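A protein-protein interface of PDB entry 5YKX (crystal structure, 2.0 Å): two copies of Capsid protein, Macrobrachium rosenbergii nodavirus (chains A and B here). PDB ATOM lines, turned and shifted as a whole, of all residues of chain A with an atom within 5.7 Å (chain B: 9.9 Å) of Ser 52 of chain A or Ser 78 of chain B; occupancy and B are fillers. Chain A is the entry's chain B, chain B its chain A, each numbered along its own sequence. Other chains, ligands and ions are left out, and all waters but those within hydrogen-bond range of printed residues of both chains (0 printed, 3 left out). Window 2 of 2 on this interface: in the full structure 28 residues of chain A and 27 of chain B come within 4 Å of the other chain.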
ATOM      1  N   ARG A  50     -32.639 -10.167  18.289  1.00  0.00           N
ATOM      2  CA  ARG A  50     -33.058  -8.825  17.777  1.00  0.00           C
ATOM      3  C   ARG A  50     -31.994  -8.235  16.936  1.00  0.00           C
ATOM      4  O   ARG A  50     -30.822  -8.061  17.352  1.00  0.00           O
ATOM      5  CB  ARG A  50     -33.325  -7.885  18.965  1.00  0.00           C
ATOM      6  CG  ARG A  50     -33.918  -6.540  18.615  1.00  0.00           C
ATOM      7  CD  ARG A  50     -34.015  -5.667  19.869  1.00  0.00           C
ATOM      8  NE  ARG A  50     -34.534  -4.343  19.691  1.00  0.00           N
ATOM      9  CZ  ARG A  50     -33.821  -3.270  19.390  1.00  0.00           C
ATOM     10  NH1 ARG A  50     -32.544  -3.409  19.122  1.00  0.00           N
ATOM     11  NH2 ARG A  50     -34.393  -2.071  19.368  1.00  0.00           N
ATOM     12  N   VAL A  51     -32.358  -7.912  15.692  1.00  0.00           N
ATOM     13  CA  VAL A  51     -31.433  -7.178  14.864  1.00  0.00           C
ATOM     14  C   VAL A  51     -31.143  -5.780  15.383  1.00  0.00           C
ATOM     15  O   VAL A  51     -32.074  -5.069  15.715  1.00  0.00           O
ATOM     16  CB  VAL A  51     -31.976  -7.122  13.419  1.00  0.00           C
ATOM     17  CG1 VAL A  51     -31.097  -6.249  12.575  1.00  0.00           C
ATOM     18  CG2 VAL A  51     -32.001  -8.526  12.850  1.00  0.00           C
ATOM     19  N   SER A  52     -29.881  -5.380  15.507  1.00  0.00           N
ATOM     20  CA  SER A  52     -29.525  -4.060  16.043  1.00  0.00           C
ATOM     21  C   SER A  52     -30.027  -2.950  15.099  1.00  0.00           C
ATOM     22  O   SER A  52     -29.953  -3.116  13.874  1.00  0.00           O
ATOM     23  CB  SER A  52     -28.013  -3.920  16.231  1.00  0.00           C
ATOM     24  OG  SER A  52     -27.693  -2.547  16.439  1.00  0.00           O
ATOM     25  N   SER A  53     -30.542  -1.867  15.677  1.00  0.00           N
ATOM     26  CA  SER A  53     -30.950  -0.720  14.900  1.00  0.00           C
ATOM     27  C   SER A  53     -29.711   0.057  14.416  1.00  0.00           C
ATOM     28  O   SER A  53     -29.820   0.836  13.498  1.00  0.00           O
ATOM     29  CB  SER A  53     -31.791   0.192  15.756  1.00  0.00           C
ATOM     30  OG  SER A  53     -30.967   0.875  16.734  1.00  0.00           O
ATOM     31  N   GLU A  54     -28.587  -0.112  15.103  1.00  0.00           N
ATOM     32  CA  GLU A  54     -27.402   0.743  15.000  1.00  0.00           C
ATOM     33  C   GLU A  54     -27.654   2.242  15.178  1.00  0.00           C
ATOM     34  O   GLU A  54     -26.850   3.003  14.757  1.00  0.00           O
ATOM     35  CB  GLU A  54     -26.694   0.584  13.645  1.00  0.00           C
ATOM     36  CG  GLU A  54     -26.270  -0.833  13.369  1.00  0.00           C
ATOM     37  CD  GLU A  54     -25.291  -0.888  12.180  1.00  0.00           C
ATOM     38  OE1 GLU A  54     -25.523  -0.401  11.049  1.00  0.00           O
ATOM     39  OE2 GLU A  54     -24.224  -1.419  12.430  1.00  0.00           O
ATOM     40  N   VAL A  55     -28.734   2.644  15.812  1.00  0.00           N
ATOM     41  CA  VAL A  55     -28.951   4.060  16.138  1.00  0.00           C
ATOM     42  C   VAL A  55     -29.150   4.319  17.639  1.00  0.00           C
ATOM     43  O   VAL A  55     -29.962   5.171  18.034  1.00  0.00           O
ATOM     44  CB  VAL A  55     -30.085   4.670  15.311  1.00  0.00           C
ATOM     45  CG1 VAL A  55     -29.693   4.698  13.813  1.00  0.00           C
ATOM     46  CG2 VAL A  55     -31.392   3.899  15.455  1.00  0.00           C
ATOM     47  N   ASP A  76     -28.236  -1.494  21.936  1.00  0.00           N
ATOM     48  CA  ASP A  76     -28.070  -2.409  20.786  1.00  0.00           C
ATOM     49  C   ASP A  76     -26.918  -2.037  19.862  1.00  0.00           C
ATOM     50  O   ASP A  76     -26.722  -2.721  18.878  1.00  0.00           O
ATOM     51  CB  ASP A  76     -29.351  -2.490  19.970  1.00  0.00           C
ATOM     52  CG  ASP A  76     -29.730  -1.129  19.279  1.00  0.00           C
ATOM     53  OD1 ASP A  76     -29.149  -0.039  19.623  1.00  0.00           O
ATOM     54  OD2 ASP A  76     -30.714  -1.151  18.499  1.00  0.00           O
ATOM     55  N   THR A  77     -26.117  -1.014  20.172  1.00  0.00           N
ATOM     56  CA  THR A  77     -25.158  -0.479  19.165  1.00  0.00           C
ATOM     57  C   THR A  77     -23.736  -0.496  19.683  1.00  0.00           C
ATOM     58  O   THR A  77     -23.365   0.246  20.607  1.00  0.00           O
ATOM     59  CB  THR A  77     -25.589   0.943  18.720  1.00  0.00           C
ATOM     60  OG1 THR A  77     -26.943   0.910  18.197  1.00  0.00           O
ATOM     61  CG2 THR A  77     -24.642   1.558  17.713  1.00  0.00           C
ATOM     62  N   SER A  78     -23.010  -1.481  19.156  1.00  0.00           N
ATOM     63  CA  SER A  78     -21.644  -1.755  19.439  1.00  0.00           C
ATOM     64  C   SER A  78     -21.307  -2.216  20.847  1.00  0.00           C
ATOM     65  O   SER A  78     -20.861  -3.388  21.052  1.00  0.00           O
ATOM     66  CB  SER A  78     -20.775  -0.564  18.871  1.00  0.00           C
ATOM     67  OG  SER A  78     -19.484  -0.893  19.242  1.00  0.00           O
ATOM     68  N   LYS A 111     -37.755  -1.918  16.875  1.00  0.00           N
ATOM     69  CA  LYS A 111     -38.088  -3.240  17.343  1.00  0.00           C
ATOM     70  C   LYS A 111     -38.078  -3.270  18.899  1.00  0.00           C
ATOM     71  O   LYS A 111     -37.206  -2.663  19.524  1.00  0.00           O
ATOM     72  CB  LYS A 111     -37.054  -4.208  16.913  1.00  0.00           C
ATOM     73  CG  LYS A 111     -37.029  -4.390  15.391  1.00  0.00           C
ATOM     74  CD  LYS A 111     -35.876  -5.333  14.988  1.00  0.00           C
ATOM     75  CE  LYS A 111     -35.313  -4.974  13.627  1.00  0.00           C
ATOM     76  NZ  LYS A 111     -36.210  -5.625  12.669  1.00  0.00           N
ATOM     77  N   MET B  48     -25.460  -9.726  28.662  1.00  0.00           N
ATOM     78  CA  MET B  48     -24.437  -9.095  27.871  1.00  0.00           C
ATOM     79  C   MET B  48     -24.115  -7.726  28.395  1.00  0.00           C
ATOM     80  O   MET B  48     -24.965  -6.854  28.689  1.00  0.00           O
ATOM     81  CB  MET B  48     -24.913  -9.114  26.356  1.00  0.00           C
ATOM     82  CG  MET B  48     -23.702  -8.874  25.472  1.00  0.00           C
ATOM     83  SD  MET B  48     -24.255  -9.493  23.609  1.00  0.00           S
ATOM     84  CE  MET B  48     -24.234 -11.443  23.696  1.00  0.00           C
ATOM     85  N   ARG B  50     -20.946  -6.029  26.755  1.00  0.00           N
ATOM     86  CA  ARG B  50     -19.848  -6.484  25.958  1.00  0.00           C
ATOM     87  C   ARG B  50     -19.806  -5.843  24.587  1.00  0.00           C
ATOM     88  O   ARG B  50     -20.794  -5.916  23.850  1.00  0.00           O
ATOM     89  CB  ARG B  50     -20.009  -8.007  25.784  1.00  0.00           C
ATOM     90  CG  ARG B  50     -18.945  -8.723  24.961  1.00  0.00           C
ATOM     91  CD  ARG B  50     -19.329 -10.222  24.844  1.00  0.00           C
ATOM     92  NE  ARG B  50     -18.374 -11.051  24.137  1.00  0.00           N
ATOM     93  CZ  ARG B  50     -18.268 -11.150  22.813  1.00  0.00           C
ATOM     94  NH1 ARG B  50     -19.032 -10.425  21.996  1.00  0.00           N
ATOM     95  NH2 ARG B  50     -17.378 -11.979  22.289  1.00  0.00           N
ATOM     96  N   SER B  52     -19.214  -5.766  20.820  1.00  0.00           N
ATOM     97  CA  SER B  52     -19.333  -6.756  19.773  1.00  0.00           C
ATOM     98  C   SER B  52     -17.949  -6.894  19.081  1.00  0.00           C
ATOM     99  O   SER B  52     -17.268  -5.877  18.850  1.00  0.00           O
ATOM    100  CB  SER B  52     -20.313  -6.325  18.693  1.00  0.00           C
ATOM    101  OG  SER B  52     -20.225  -7.209  17.549  1.00  0.00           O
ATOM    102  N   SER B  53     -17.582  -8.104  18.729  1.00  0.00           N
ATOM    103  CA  SER B  53     -16.334  -8.314  17.986  1.00  0.00           C
ATOM    104  C   SER B  53     -16.560  -7.927  16.528  1.00  0.00           C
ATOM    105  O   SER B  53     -15.608  -7.753  15.802  1.00  0.00           O
ATOM    106  CB  SER B  53     -15.994  -9.786  18.039  1.00  0.00           C
ATOM    107  OG  SER B  53     -16.947 -10.586  17.309  1.00  0.00           O
ATOM    108  N   GLU B  54     -17.814  -8.001  16.094  1.00  0.00           N
ATOM    109  CA  GLU B  54     -18.258  -7.970  14.696  1.00  0.00           C
ATOM    110  C   GLU B  54     -17.639  -9.038  13.854  1.00  0.00           C
ATOM    111  O   GLU B  54     -17.582  -8.900  12.664  1.00  0.00           O
ATOM    112  CB  GLU B  54     -17.933  -6.644  14.035  1.00  0.00           C
ATOM    113  CG  GLU B  54     -18.356  -5.430  14.780  1.00  0.00           C
ATOM    114  CD  GLU B  54     -18.206  -4.160  13.892  1.00  0.00           C
ATOM    115  OE1 GLU B  54     -17.157  -3.641  13.544  1.00  0.00           O
ATOM    116  OE2 GLU B  54     -19.210  -3.662  13.507  1.00  0.00           O
ATOM    117  N   VAL B  55     -17.141 -10.117  14.454  1.00  0.00           N
ATOM    118  CA  VAL B  55     -16.676 -11.221  13.663  1.00  0.00           C
ATOM    119  C   VAL B  55     -17.423 -12.514  13.940  1.00  0.00           C
ATOM    120  O   VAL B  55     -16.858 -13.626  13.854  1.00  0.00           O
ATOM    121  CB  VAL B  55     -15.134 -11.367  13.731  1.00  0.00           C
ATOM    122  CG1 VAL B  55     -14.496 -10.173  13.045  1.00  0.00           C
ATOM    123  CG2 VAL B  55     -14.632 -11.539  15.146  1.00  0.00           C
ATOM    124  N   LEU B  56     -18.733 -12.391  14.213  1.00  0.00           N
ATOM    125  CA  LEU B  56     -19.687 -13.493  14.136  1.00  0.00           C
ATOM    126  C   LEU B  56     -19.351 -14.605  15.136  1.00  0.00           C
ATOM    127  O   LEU B  56     -19.032 -15.758  14.795  1.00  0.00           O
ATOM    128  CB  LEU B  56     -19.817 -14.021  12.683  1.00  0.00           C
ATOM    129  CG  LEU B  56     -20.582 -13.066  11.743  1.00  0.00           C
ATOM    130  CD1 LEU B  56     -19.565 -12.160  11.198  1.00  0.00           C
ATOM    131  CD2 LEU B  56     -21.274 -13.779  10.591  1.00  0.00           C
ATOM    132  N   GLN B  57     -19.287 -14.217  16.394  1.00  0.00           N
ATOM    133  CA  GLN B  57     -18.812 -15.168  17.410  1.00  0.00           C
ATOM    134  C   GLN B  57     -20.026 -15.854  17.995  1.00  0.00           C
ATOM    135  O   GLN B  57     -20.754 -15.280  18.845  1.00  0.00           O
ATOM    136  CB  GLN B  57     -17.957 -14.442  18.444  1.00  0.00           C
ATOM    137  CG  GLN B  57     -16.692 -13.843  17.849  1.00  0.00           C
ATOM    138  CD  GLN B  57     -15.751 -13.207  18.799  1.00  0.00           C
ATOM    139  OE1 GLN B  57     -16.123 -12.620  19.814  1.00  0.00           O
ATOM    140  NE2 GLN B  57     -14.451 -13.186  18.400  1.00  0.00           N
ATOM    141  N   PHE B  75     -24.711 -14.537  20.283  1.00  0.00           N
ATOM    142  CA  PHE B  75     -24.221 -14.107  18.956  1.00  0.00           C
ATOM    143  C   PHE B  75     -24.132 -12.609  18.986  1.00  0.00           C
ATOM    144  O   PHE B  75     -25.070 -11.936  19.482  1.00  0.00           O
ATOM    145  CB  PHE B  75     -25.169 -14.563  17.806  1.00  0.00           C
ATOM    146  CG  PHE B  75     -24.527 -14.444  16.452  1.00  0.00           C
ATOM    147  CD1 PHE B  75     -23.599 -15.396  16.064  1.00  0.00           C
ATOM    148  CD2 PHE B  75     -24.810 -13.429  15.582  1.00  0.00           C
ATOM    149  CE1 PHE B  75     -22.990 -15.348  14.813  1.00  0.00           C
ATOM    150  CE2 PHE B  75     -24.220 -13.389  14.327  1.00  0.00           C
ATOM    151  CZ  PHE B  75     -23.286 -14.326  13.944  1.00  0.00           C
ATOM    152  N   ASP B  76     -22.993 -12.050  18.542  1.00  0.00           N
ATOM    153  CA  ASP B  76     -22.737 -10.654  18.767  1.00  0.00           C
ATOM    154  C   ASP B  76     -22.783  -9.719  17.515  1.00  0.00           C
ATOM    155  O   ASP B  76     -22.491  -8.510  17.624  1.00  0.00           O
ATOM    156  CB  ASP B  76     -21.361 -10.450  19.475  1.00  0.00           C
ATOM    157  CG  ASP B  76     -20.131 -10.838  18.593  1.00  0.00           C
ATOM    158  OD1 ASP B  76     -20.272 -11.497  17.531  1.00  0.00           O
ATOM    159  OD2 ASP B  76     -18.973 -10.590  19.054  1.00  0.00           O
ATOM    160  N   THR B  77     -23.155 -10.223  16.356  1.00  0.00           N
ATOM    161  CA  THR B  77     -22.904  -9.418  15.116  1.00  0.00           C
ATOM    162  C   THR B  77     -24.198  -9.241  14.360  1.00  0.00           C
ATOM    163  O   THR B  77     -24.796 -10.209  13.886  1.00  0.00           O
ATOM    164  CB  THR B  77     -21.816 -10.094  14.222  1.00  0.00           C
ATOM    165  OG1 THR B  77     -20.593 -10.144  14.962  1.00  0.00           O
ATOM    166  CG2 THR B  77     -21.579  -9.230  12.969  1.00  0.00           C
ATOM    167  N   SER B  78     -24.698  -8.015  14.383  1.00  0.00           N
ATOM    168  CA  SER B  78     -25.940  -7.600  13.748  1.00  0.00           C
ATOM    169  C   SER B  78     -27.223  -8.218  14.288  1.00  0.00           C
ATOM    170  O   SER B  78     -28.034  -7.508  14.845  1.00  0.00           O
ATOM    171  CB  SER B  78     -25.931  -7.956  12.300  1.00  0.00           C
ATOM    172  OG  SER B  78     -24.874  -7.321  11.690  1.00  0.00           O
ATOM    173  N   ALA B  79     -27.400  -9.521  14.127  1.00  0.00           N
ATOM    174  CA  ALA B  79     -28.524 -10.204  14.664  1.00  0.00           C
ATOM    175  C   ALA B  79     -28.139 -10.693  16.094  1.00  0.00           C
ATOM    176  O   ALA B  79     -27.610 -11.829  16.275  1.00  0.00           O
ATOM    177  CB  ALA B  79     -28.927 -11.368  13.791  1.00  0.00           C
ATOM    178  N   ILE B  80     -28.404  -9.860  17.099  1.00  0.00           N
ATOM    179  CA  ILE B  80     -27.852 -10.088  18.440  1.00  0.00           C
ATOM    180  C   ILE B  80     -28.645 -11.188  19.124  1.00  0.00           C
ATOM    181  O   ILE B  80     -29.876 -11.131  19.104  1.00  0.00           O
ATOM    182  CB  ILE B  80     -27.927  -8.839  19.258  1.00  0.00           C
ATOM    183  CG1 ILE B  80     -27.117  -7.764  18.510  1.00  0.00           C
ATOM    184  CG2 ILE B  80     -27.293  -9.084  20.620  1.00  0.00           C
ATOM    185  CD1 ILE B  80     -27.244  -6.362  19.000  1.00  0.00           C
ATOM    186  N   LYS B  81     -27.937 -12.173  19.654  1.00  0.00           N
ATOM    187  CA  LYS B  81     -28.555 -13.246  20.396  1.00  0.00           C
ATOM    188  C   LYS B  81     -27.946 -13.284  21.792  1.00  0.00           C
ATOM    189  O   LYS B  81     -26.727 -13.364  21.959  1.00  0.00           O
ATOM    190  CB  LYS B  81     -28.319 -14.573  19.695  1.00  0.00           C
ATOM    191  CG  LYS B  81     -29.243 -15.668  20.074  1.00  0.00           C
ATOM    192  CD  LYS B  81     -30.375 -15.838  19.052  1.00  0.00           C
ATOM    193  CE  LYS B  81     -31.046 -17.208  19.161  1.00  0.00           C
ATOM    194  NZ  LYS B  81     -32.378 -17.131  19.853  1.00  0.00           N
ATOM    195  N   CYS B  82     -28.836 -13.246  22.769  1.00  0.00           N
ATOM    196  CA  CYS B  82     -28.521 -13.433  24.186  1.00  0.00           C
ATOM    197  C   CYS B  82     -29.712 -14.108  24.782  1.00  0.00           C
ATOM    198  O   CYS B  82     -30.643 -13.449  25.292  1.00  0.00           O
ATOM    199  CB  CYS B  82     -28.278 -12.043  24.839  1.00  0.00           C
ATOM    200  SG  CYS B  82     -27.752 -12.122  26.590  1.00  0.00           S
ATOM    201  N   TYR B 113     -18.186 -14.460  26.687  1.00  0.00           N
ATOM    202  CA  TYR B 113     -19.588 -14.280  26.904  1.00  0.00           C
ATOM    203  C   TYR B 113     -19.868 -14.482  28.402  1.00  0.00           C
ATOM    204  O   TYR B 113     -19.017 -15.026  29.126  1.00  0.00           O
ATOM    205  CB  TYR B 113     -20.405 -15.212  26.014  1.00  0.00           C
ATOM    206  CG  TYR B 113     -20.408 -14.727  24.577  1.00  0.00           C
ATOM    207  CD1 TYR B 113     -20.994 -13.522  24.244  1.00  0.00           C
ATOM    208  CD2 TYR B 113     -19.936 -15.534  23.548  1.00  0.00           C
ATOM    209  CE1 TYR B 113     -21.035 -13.085  22.962  1.00  0.00           C
ATOM    210  CE2 TYR B 113     -19.920 -15.072  22.250  1.00  0.00           C
ATOM    211  CZ  TYR B 113     -20.514 -13.874  21.971  1.00  0.00           C
ATOM    212  OH  TYR B 113     -20.622 -13.374  20.724  1.00  0.00           O
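Of the 10 printed residues of chain A, 5 touch a printed residue of chain B. Of the 17 printed residues of chain B, 5 touch a printed residue of chain A. Printed residues of chain B that touch a printed residue of chain A: Arg 50, Ser 52, Ser 78, Ala 79 and Ile 80. Hydrophobic or aromatic side chains of chain B within 4 Å of the printed part of chain A: Ile 80. Among the printed residues, 9 pairs touch across the chains.
Among the printed residues, pairs that only touch across the chains: Arg 50 of chain A with Ser 78 of chain B (3.8 Å), Arg 50 of chain A with Ala 79 of chain B (3.96 Å), Val 51 of chain A with Ser 78 of chain B (3.4 Å), Ser 52 of chain A with Ile 80 of chain B (3.8 Å), Asp 76 of chain A with Ile 80 of chain B (3.7 Å) and Ser 78 of chain A with Arg 50 of chain B (3.8 Å).
The side-chain amide oxygen (OE1) of Gln 57 of chain B is in hydrogen-bond range of the guanidinium group (NH2) of Arg 50 of chain B, at 2.8 Å. OD2 of Asp 76 of chain B lies within salt-bridge range of NH1 of Arg 50 of chain B, at 2.9 Å. The guanidinium group of Arg 50 of chain A is in salt-bridge range of the side-chain carboxylate of Asp 76 of chain A, at 3.0 Å. NH2 of Arg 50 of chain A lies within hydrogen-bond range of O of Lys 111 of chain A (2.9 Å). The backbone NH of Glu 54 of chain A is in hydrogen-bond range of the side-chain hydroxyl of Ser 52 of chain A. The side-chain carboxylate (OD1) of Asp 76 of chain A lies within hydrogen-bond range of the side-chain hydroxyl (OG1) of Thr 77 of chain A, at 2.8 Å.
Arg 50 of chain A touches Ser 78 of chain B, and with the chains exchanged Ser 78 of chain A touches Arg 50 of chain B. Ser 52 of chain A touches Ser 78 of chain B, and with the chains exchanged Ser 78 of chain A touches Ser 52 of chain B. Positions printed for both chains: 50, 52, 53, 54, 55, 76, 77 and 78. Of the 9 pairs that touch across the chains among the printed residues, 4 have their exchanged pair printed and touching as well.
O of Ser 78 of chain A sits at hydrogen-bond distance from N of Ser 52 of chain B (2.9 Å). O of Ser 78 of chain B is in hydrogen-bond range of N of Ser 52 of chain A (2.9 Å). The backbone NH (N) of Ile 80 of chain B sits at hydrogen-bond distance from the backbone carbonyl oxygen (O) of Arg 50 of chain A (3.0 Å).
Printed residues of chain B within 4 Å of Arg 50 of chain A: Ser 78, Ala 79 and Ile 80. Val 51 of chain A touches just one residue of chain B: Ser 78 (3.4 Å). Of chain B, only Ser 78 (2.9 Å) and Ile 80 (3.8 Å) come within 4 Å of Ser 52 of chain A. No residue of chain B comes within 4 Å of Ser 53 of chain A. Glu 54 of chain A touches none of the printed residues of chain B. Of chain B, only Ile 80 (3.7 Å) comes within 4 Å of Asp 76 of chain A. Printed residues of chain B within 4 Å of Ser 78 of chain A: Arg 50 (3.8 Å) and Ser 52 (2.9 Å). Val 55 of chain B touches none of the printed residues of chain A. Ser 78 of chain B touches just these residues of chain A: Arg 50, Val 51 and Ser 52. The nearest residue of chain B that does not touch Ser 52 of chain A is Ala 79 of chain B (5.0 Å). The nearest printed residue of chain A that does not touch Ser 78 of chain B is Glu 54 of chain A (6.0 Å).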
